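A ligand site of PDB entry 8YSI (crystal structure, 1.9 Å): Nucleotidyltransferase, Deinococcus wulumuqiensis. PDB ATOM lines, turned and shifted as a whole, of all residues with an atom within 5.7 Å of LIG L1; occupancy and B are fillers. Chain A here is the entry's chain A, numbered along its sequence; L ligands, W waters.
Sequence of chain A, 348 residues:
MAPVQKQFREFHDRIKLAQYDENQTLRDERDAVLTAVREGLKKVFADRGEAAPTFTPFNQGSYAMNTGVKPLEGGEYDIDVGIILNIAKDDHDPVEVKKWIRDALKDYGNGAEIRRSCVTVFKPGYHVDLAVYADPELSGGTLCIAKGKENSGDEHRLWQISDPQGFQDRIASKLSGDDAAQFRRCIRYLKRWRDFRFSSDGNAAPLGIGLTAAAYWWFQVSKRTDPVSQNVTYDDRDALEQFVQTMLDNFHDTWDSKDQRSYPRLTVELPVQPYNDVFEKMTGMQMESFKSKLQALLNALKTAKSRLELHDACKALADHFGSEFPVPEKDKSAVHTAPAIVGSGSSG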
ATOM      1  N   GLN A  60     -12.969 -19.283   9.099  1.00  0.00           N
ATOM      2  CA  GLN A  60     -11.973 -18.201   9.305  1.00  0.00           C
ATOM      3  C   GLN A  60     -12.689 -16.926   9.728  1.00  0.00           C
ATOM      4  O   GLN A  60     -13.937 -16.891   9.606  1.00  0.00           O
ATOM      5  CB  GLN A  60     -11.209 -17.886   8.024  1.00  0.00           C
ATOM      6  CG  GLN A  60     -10.295 -19.009   7.605  1.00  0.00           C
ATOM      7  CD  GLN A  60      -9.272 -18.559   6.600  1.00  0.00           C
ATOM      8  OE1 GLN A  60      -8.829 -19.330   5.775  1.00  0.00           O
ATOM      9  NE2 GLN A  60      -8.854 -17.318   6.698  1.00  0.00           N
ATOM     10  N   ASP A  78     -19.659 -10.617   5.635  1.00  0.00           N
ATOM     11  CA  ASP A  78     -18.354 -11.131   5.156  1.00  0.00           C
ATOM     12  C   ASP A  78     -18.175 -12.553   5.696  1.00  0.00           C
ATOM     13  O   ASP A  78     -17.747 -12.702   6.857  1.00  0.00           O
ATOM     14  CB  ASP A  78     -17.208 -10.225   5.611  1.00  0.00           C
ATOM     15  CG  ASP A  78     -15.837 -10.851   5.464  1.00  0.00           C
ATOM     16  OD1 ASP A  78     -15.638 -11.585   4.456  1.00  0.00           O
ATOM     17  OD2 ASP A  78     -14.973 -10.604   6.326  1.00  0.00           O
ATOM     18  N   ASP A  80     -16.095 -15.719   5.882  1.00  0.00           N
ATOM     19  CA  ASP A  80     -14.695 -16.157   5.615  1.00  0.00           C
ATOM     20  C   ASP A  80     -14.584 -17.668   5.826  1.00  0.00           C
ATOM     21  O   ASP A  80     -14.951 -18.166   6.917  1.00  0.00           O
ATOM     22  CB  ASP A  80     -13.686 -15.390   6.452  1.00  0.00           C
ATOM     23  CG  ASP A  80     -13.885 -13.902   6.383  1.00  0.00           C
ATOM     24  OD1 ASP A  80     -14.127 -13.298   7.449  1.00  0.00           O
ATOM     25  OD2 ASP A  80     -13.828 -13.335   5.237  1.00  0.00           O
ATOM     26  N   ARG A 115      -8.897 -12.531  -6.099  1.00  0.00           N
ATOM     27  CA  ARG A 115      -8.276 -11.390  -5.375  1.00  0.00           C
ATOM     28  C   ARG A 115      -6.876 -11.787  -4.894  1.00  0.00           C
ATOM     29  O   ARG A 115      -6.523 -12.958  -4.978  1.00  0.00           O
ATOM     30  CB  ARG A 115      -9.133 -11.002  -4.184  1.00  0.00           C
ATOM     31  CG  ARG A 115     -10.593 -10.739  -4.532  1.00  0.00           C
ATOM     32  CD  ARG A 115     -11.236 -10.136  -3.305  1.00  0.00           C
ATOM     33  NE  ARG A 115     -12.095  -9.010  -3.615  1.00  0.00           N
ATOM     34  CZ  ARG A 115     -12.256  -7.959  -2.821  1.00  0.00           C
ATOM     35  NH1 ARG A 115     -11.599  -7.878  -1.672  1.00  0.00           N
ATOM     36  NH2 ARG A 115     -13.049  -6.970  -3.192  1.00  0.00           N
ATOM     37  N   ARG A 116      -6.135 -10.831  -4.338  1.00  0.00           N
ATOM     38  CA  ARG A 116      -4.724 -11.036  -3.962  1.00  0.00           C
ATOM     39  C   ARG A 116      -4.652 -12.240  -3.016  1.00  0.00           C
ATOM     40  O   ARG A 116      -3.733 -13.052  -3.206  1.00  0.00           O
ATOM     41  CB  ARG A 116      -4.145  -9.740  -3.390  1.00  0.00           C
ATOM     42  CG  ARG A 116      -3.693  -8.781  -4.481  1.00  0.00           C
ATOM     43  CD  ARG A 116      -3.293  -7.382  -4.007  1.00  0.00           C
ATOM     44  NE  ARG A 116      -2.023  -6.963  -4.622  1.00  0.00           N
ATOM     45  CZ  ARG A 116      -1.534  -5.714  -4.594  1.00  0.00           C
ATOM     46  NH1 ARG A 116      -2.191  -4.734  -4.008  1.00  0.00           N
ATOM     47  NH2 ARG A 116      -0.362  -5.471  -5.171  1.00  0.00           N
ATOM     48  N   SER A 117      -5.627 -12.405  -2.106  1.00  0.00           N
ATOM     49  CA  SER A 117      -5.552 -13.409  -0.999  1.00  0.00           C
ATOM     50  C   SER A 117      -6.725 -14.398  -0.983  1.00  0.00           C
ATOM     51  O   SER A 117      -6.755 -15.281  -0.097  1.00  0.00           O
ATOM     52  CB  SER A 117      -5.429 -12.671   0.313  1.00  0.00           C
ATOM     53  OG  SER A 117      -4.300 -11.825   0.281  1.00  0.00           O
ATOM     54  N   CYS A 118      -7.671 -14.296  -1.902  1.00  0.00           N
ATOM     55  CA  CYS A 118      -8.843 -15.195  -1.888  1.00  0.00           C
ATOM     56  C   CYS A 118      -9.526 -15.203  -3.255  1.00  0.00           C
ATOM     57  O   CYS A 118      -9.130 -14.414  -4.147  1.00  0.00           O
ATOM     58  CB  CYS A 118      -9.847 -14.832  -0.795  1.00  0.00           C
ATOM     59  SG  CYS A 118     -10.649 -13.212  -1.020  1.00  0.00           S
ATOM     60  N   THR A 120     -13.350 -14.409  -4.093  1.00  0.00           N
ATOM     61  CA  THR A 120     -14.602 -13.833  -3.532  1.00  0.00           C
ATOM     62  C   THR A 120     -15.761 -14.095  -4.490  1.00  0.00           C
ATOM     63  O   THR A 120     -15.650 -13.707  -5.684  1.00  0.00           O
ATOM     64  CB  THR A 120     -14.479 -12.314  -3.288  1.00  0.00           C
ATOM     65  OG1 THR A 120     -13.286 -12.055  -2.549  1.00  0.00           O
ATOM     66  CG2 THR A 120     -15.666 -11.759  -2.537  1.00  0.00           C
ATOM     67  N   ASP A 129     -15.580 -15.048   1.087  1.00  0.00           N
ATOM     68  CA  ASP A 129     -14.145 -14.939   0.788  1.00  0.00           C
ATOM     69  C   ASP A 129     -13.525 -16.305   1.047  1.00  0.00           C
ATOM     70  O   ASP A 129     -13.510 -16.714   2.228  1.00  0.00           O
ATOM     71  CB  ASP A 129     -13.487 -13.856   1.638  1.00  0.00           C
ATOM     72  CG  ASP A 129     -13.866 -12.445   1.229  1.00  0.00           C
ATOM     73  OD1 ASP A 129     -14.372 -12.294   0.089  1.00  0.00           O
ATOM     74  OD2 ASP A 129     -13.612 -11.517   2.029  1.00  0.00           O
ATOM     75  N   ALA A 131     -10.341 -18.384   1.126  1.00  0.00           N
ATOM     76  CA  ALA A 131      -8.891 -18.554   1.216  1.00  0.00           C
ATOM     77  C   ALA A 131      -8.583 -19.956   0.707  1.00  0.00           C
ATOM     78  O   ALA A 131      -9.226 -20.934   1.150  1.00  0.00           O
ATOM     79  CB  ALA A 131      -8.438 -18.337   2.618  1.00  0.00           C
ATOM     80  N   TYR A 133      -5.728 -22.882   0.103  1.00  0.00           N
ATOM     81  CA  TYR A 133      -4.459 -23.412   0.633  1.00  0.00           C
ATOM     82  C   TYR A 133      -4.100 -24.735  -0.049  1.00  0.00           C
ATOM     83  O   TYR A 133      -4.988 -25.472  -0.445  1.00  0.00           O
ATOM     84  CB  TYR A 133      -4.554 -23.638   2.145  1.00  0.00           C
ATOM     85  CG  TYR A 133      -4.998 -22.414   2.927  1.00  0.00           C
ATOM     86  CD1 TYR A 133      -6.342 -22.145   3.093  1.00  0.00           C
ATOM     87  CD2 TYR A 133      -4.092 -21.552   3.509  1.00  0.00           C
ATOM     88  CE1 TYR A 133      -6.787 -21.050   3.838  1.00  0.00           C
ATOM     89  CE2 TYR A 133      -4.510 -20.437   4.213  1.00  0.00           C
ATOM     90  CZ  TYR A 133      -5.868 -20.187   4.393  1.00  0.00           C
ATOM     91  OH  TYR A 133      -6.305 -19.087   5.099  1.00  0.00           O
ATOM     92  N   ILE A 145      -1.127 -20.219   1.616  1.00  0.00           N
ATOM     93  CA  ILE A 145      -2.260 -19.532   0.964  1.00  0.00           C
ATOM     94  C   ILE A 145      -1.801 -19.115  -0.449  1.00  0.00           C
ATOM     95  O   ILE A 145      -0.601 -18.719  -0.612  1.00  0.00           O
ATOM     96  CB  ILE A 145      -2.774 -18.360   1.840  1.00  0.00           C
ATOM     97  CG1 ILE A 145      -4.135 -17.844   1.378  1.00  0.00           C
ATOM     98  CG2 ILE A 145      -1.753 -17.230   1.944  1.00  0.00           C
ATOM     99  CD1 ILE A 145      -4.855 -16.966   2.386  1.00  0.00           C
ATOM    100  N   LYS A 147      -1.458 -16.622  -3.117  1.00  0.00           N
ATOM    101  CA  LYS A 147      -1.379 -15.137  -3.240  1.00  0.00           C
ATOM    102  C   LYS A 147      -1.010 -14.741  -4.674  1.00  0.00           C
ATOM    103  O   LYS A 147      -0.188 -15.433  -5.285  1.00  0.00           O
ATOM    104  CB  LYS A 147      -0.324 -14.529  -2.309  1.00  0.00           C
ATOM    105  CG  LYS A 147      -0.641 -14.594  -0.820  1.00  0.00           C
ATOM    106  CD  LYS A 147      -1.803 -13.703  -0.382  1.00  0.00           C
ATOM    107  CE  LYS A 147      -1.378 -12.596   0.568  1.00  0.00           C
ATOM    108  NZ  LYS A 147      -0.505 -11.600  -0.102  1.00  0.00           N
ATOM    109  N   LYS A 149      -2.723 -12.217  -8.344  1.00  0.00           N
ATOM    110  CA  LYS A 149      -3.796 -12.125  -9.362  1.00  0.00           C
ATOM    111  C   LYS A 149      -3.142 -12.379 -10.718  1.00  0.00           C
ATOM    112  O   LYS A 149      -1.906 -12.476 -10.747  1.00  0.00           O
ATOM    113  CB  LYS A 149      -4.436 -10.733  -9.384  1.00  0.00           C
ATOM    114  CG  LYS A 149      -5.076 -10.266  -8.087  1.00  0.00           C
ATOM    115  CD  LYS A 149      -6.206  -9.259  -8.292  1.00  0.00           C
ATOM    116  CE  LYS A 149      -6.184  -8.106  -7.300  1.00  0.00           C
ATOM    117  NZ  LYS A 149      -4.948  -7.303  -7.433  1.00  0.00           N
ATOM    118  N   GLN A 160       2.177 -18.405   0.049  1.00  0.00           N
ATOM    119  CA  GLN A 160       2.697 -17.725   1.268  1.00  0.00           C
ATOM    120  C   GLN A 160       2.340 -18.530   2.496  1.00  0.00           C
ATOM    121  O   GLN A 160       1.147 -18.827   2.675  1.00  0.00           O
ATOM    122  CB  GLN A 160       2.144 -16.315   1.387  1.00  0.00           C
ATOM    123  CG  GLN A 160       2.853 -15.483   2.449  1.00  0.00           C
ATOM    124  CD  GLN A 160       2.270 -14.108   2.630  1.00  0.00           C
ATOM    125  OE1 GLN A 160       1.050 -13.921   2.699  1.00  0.00           O
ATOM    126  NE2 GLN A 160       3.148 -13.143   2.768  1.00  0.00           N
ATOM    127  N   SER A 162       1.051 -19.295   6.007  1.00  0.00           N
ATOM    128  CA  SER A 162      -0.194 -18.746   6.580  1.00  0.00           C
ATOM    129  C   SER A 162      -0.532 -19.531   7.839  1.00  0.00           C
ATOM    130  O   SER A 162      -0.131 -20.738   7.923  1.00  0.00           O
ATOM    131  CB  SER A 162      -1.314 -18.846   5.560  1.00  0.00           C
ATOM    132  OG  SER A 162      -2.359 -17.952   5.870  1.00  0.00           O
HETATM  133  P1  LIG L   1      -7.303  -9.595  -0.395  1.00  0.00           P
HETATM  134  O1  LIG L   1      -5.894  -9.407   0.053  1.00  0.00           O
HETATM  135  O2  LIG L   1      -7.568 -10.541  -1.522  1.00  0.00           O
HETATM  136  O3  LIG L   1      -7.905  -8.171  -0.806  1.00  0.00           O
HETATM  137  O4  LIG L   1      -8.197  -9.984   0.891  1.00  0.00           O
HETATM  138  P2  LIG L   1      -7.324  -7.263  -2.001  1.00  0.00           P
HETATM  139  O5  LIG L   1      -7.494  -7.992  -3.293  1.00  0.00           O
HETATM  140  O6  LIG L   1      -5.968  -6.805  -1.576  1.00  0.00           O
HETATM  141  O7  LIG L   1      -8.314  -6.004  -2.029  1.00  0.00           O
HETATM  142  P3  LIG L   1      -8.627  -5.040  -3.293  1.00  0.00           P
HETATM  143  O8  LIG L   1     -10.030  -5.367  -3.727  1.00  0.00           O
HETATM  144  O9  LIG L   1      -8.482  -3.618  -2.782  1.00  0.00           O
HETATM  145  O10 LIG L   1      -7.595  -5.384  -4.358  1.00  0.00           O
HETATM  146  C1  LIG L   1      -9.594 -10.320   0.728  1.00  0.00           C
HETATM  147  C2  LIG L   1      -9.965 -11.369   1.752  1.00  0.00           C
HETATM  148  O11 LIG L   1      -9.024 -12.456   1.714  1.00  0.00           O
HETATM  149  C3  LIG L   1      -9.063 -13.162   2.940  1.00  0.00           C
HETATM  150  C4  LIG L   1      -9.882 -12.318   3.924  1.00  0.00           C
HETATM  151  O12 LIG L   1     -11.186 -12.857   4.053  1.00  0.00           O
HETATM  152  C5  LIG L   1      -9.906 -10.940   3.234  1.00  0.00           C
HETATM  153  O13 LIG L   1     -11.042 -10.167   3.622  1.00  0.00           O
HETATM  154  N1  LIG L   1      -7.672 -13.397   3.408  1.00  0.00           N
HETATM  155  C6  LIG L   1      -6.706 -12.424   3.272  1.00  0.00           C
HETATM  156  C7  LIG L   1      -7.415 -14.572   4.123  1.00  0.00           C
HETATM  157  O14 LIG L   1      -8.252 -15.437   4.328  1.00  0.00           O
HETATM  158  N2  LIG L   1      -6.132 -14.691   4.583  1.00  0.00           N
HETATM  159  C8  LIG L   1      -5.104 -13.793   4.423  1.00  0.00           C
HETATM  160  O15 LIG L   1      -4.003 -14.049   4.902  1.00  0.00           O
HETATM  161  C9  LIG L   1      -5.445 -12.590   3.717  1.00  0.00           C
HETATM  162  P1  LG2 L   2     -11.009 -10.481   7.292  1.00  0.00           P
HETATM  163  O1  LG2 L   2     -10.347  -9.315   6.637  1.00  0.00           O
HETATM  164  O2  LG2 L   2     -12.303 -11.009   6.781  1.00  0.00           O
HETATM  165  O3  LG2 L   2     -11.115 -10.157   8.853  1.00  0.00           O
HETATM  166  O4  LG2 L   2      -9.947 -11.654   7.370  1.00  0.00           O
HETATM  167  P2  LG2 L   2     -12.112 -10.522  10.027  1.00  0.00           P
HETATM  168  O5  LG2 L   2     -11.278 -10.978  11.213  1.00  0.00           O
HETATM  169  O6  LG2 L   2     -13.168 -11.446   9.486  1.00  0.00           O
HETATM  170  O7  LG2 L   2     -12.745  -9.068  10.332  1.00  0.00           O
HETATM  171  P3  LG2 L   2     -14.246  -8.453   9.985  1.00  0.00           P
HETATM  172  O8  LG2 L   2     -14.188  -6.933   9.873  1.00  0.00           O
HETATM  173  O9  LG2 L   2     -14.589  -9.138   8.660  1.00  0.00           O
HETATM  174  O10 LG2 L   2     -15.168  -8.891  11.107  1.00  0.00           O
HETATM  175  C1  LG2 L   2     -10.323 -13.038   7.453  1.00  0.00           C
HETATM  176  C2  LG2 L   2      -9.137 -13.773   7.998  1.00  0.00           C
HETATM  177  O11 LG2 L   2      -8.089 -13.838   6.991  1.00  0.00           O
HETATM  178  C3  LG2 L   2      -6.818 -13.691   7.617  1.00  0.00           C
HETATM  179  C4  LG2 L   2      -7.078 -13.734   9.125  1.00  0.00           C
HETATM  180  O12 LG2 L   2      -7.087 -15.062   9.599  1.00  0.00           O
HETATM  181  C5  LG2 L   2      -8.460 -13.071   9.185  1.00  0.00           C
HETATM  182  O13 LG2 L   2      -9.252 -13.265  10.352  1.00  0.00           O
HETATM  183  N1  LG2 L   2      -6.204 -12.402   7.203  1.00  0.00           N
HETATM  184  C6  LG2 L   2      -6.946 -11.370   6.677  1.00  0.00           C
HETATM  185  C7  LG2 L   2      -4.837 -12.254   7.416  1.00  0.00           C
HETATM  186  O14 LG2 L   2      -4.134 -13.140   7.863  1.00  0.00           O
HETATM  187  N2  LG2 L   2      -4.317 -11.046   7.048  1.00  0.00           N
HETATM  188  C8  LG2 L   2      -5.002  -9.968   6.517  1.00  0.00           C
HETATM  189  O15 LG2 L   2      -4.389  -8.924   6.257  1.00  0.00           O
HETATM  190  C9  LG2 L   2      -6.404 -10.187   6.340  1.00  0.00           C
HETATM  191  O   HOH W   1      -2.102 -15.387   5.719  1.00  0.00           O
HETATM  192  O   HOH W   2      -5.531 -16.820   6.080  1.00  0.00           O
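O2 of LIG L1 lies within hydrogen-bond range of N of Ser 117, at 2.8 Å.
An oxygen (O1) of LIG L1 lies within hydrogen-bond range of the side-chain hydroxyl of Ser 117 (2.9 Å).
O12 of LIG L1 lies within hydrogen-bond range of OD2 of Asp 80.
The side-chain amide nitrogen (NE2) of Gln 60 is in hydrogen-bond range of an oxygen (O14) of LIG L1 (3.1 Å).
An oxygen (O8) of LIG L1 lies within salt-bridge range of the guanidinium group (NH2) of Arg 115.
An oxygen (O2) of LIG L1 lies within hydrogen-bond range of the backbone NH of Arg 116, at 3.2 Å.
SG of Cys 118 is in hydrogen-bond range of O11 of LIG L1, 3.3 Å away.
An oxygen (O13) of LIG L1 is in hydrogen-bond range of the side-chain carboxylate (OD2) of Asp 129 (3.3 Å).
The side-chain carboxylate (OD1) of Asp 80 sits close to an oxygen (O6) of LG2 L2 (2.9 Å).
The side-chain carboxylate of Asp 78 lies close to an oxygen (O2) of LG2 L2 (2.7 Å).
O13 of LIG L1 is in hydrogen-bond range of O1 of LG2 L2 (3.2 Å).
The backbone carbonyl oxygen (O) of Asp 80 is in hydrogen-bond range of the backbone NH (N) of Gln 60.
The side-chain carboxylate (OD2) of Asp 80 sits close to the side-chain carboxylate (OD1) of Asp 78 (2.6 Å).
The side-chain amide oxygen of Gln 60 lies within hydrogen-bond range of the side-chain hydroxyl of Tyr 133 (2.6 Å).
The guanidinium group (NE) of Arg 115 lies close to the side-chain hydroxyl (OG1) of Thr 120 (3.4 Å).
The side-chain hydroxyl of Thr 120 is in hydrogen-bond range of the side-chain sulfur of Cys 118, 3.3 Å away.
OG1 of Thr 120 sits at hydrogen-bond distance from OD1 of Asp 129 (2.9 Å).
The backbone NH (N) of Ile 145 sits at hydrogen-bond distance from the backbone carbonyl oxygen (O) of Gln 160 (2.9 Å).
Merely in contact with LIG L1: Ala 131 and Ile 145.
Hydrophobic or aromatic side chains that line LIG L1: Ala 131 and Ile 145.
Water W1 lies within hydrogen-bond range of an oxygen (O15) of LIG L1 (2.5 Å) and the side-chain hydroxyl (OG) of Ser 162 (2.6 Å).
Water W2 lies within hydrogen-bond range of the side-chain hydroxyl (OH) of Tyr 133, a nitrogen (N2) of LIG L1, the side-chain hydroxyl (OG) of Ser 162 and the side-chain amide nitrogen (NE2) of Gln 60.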
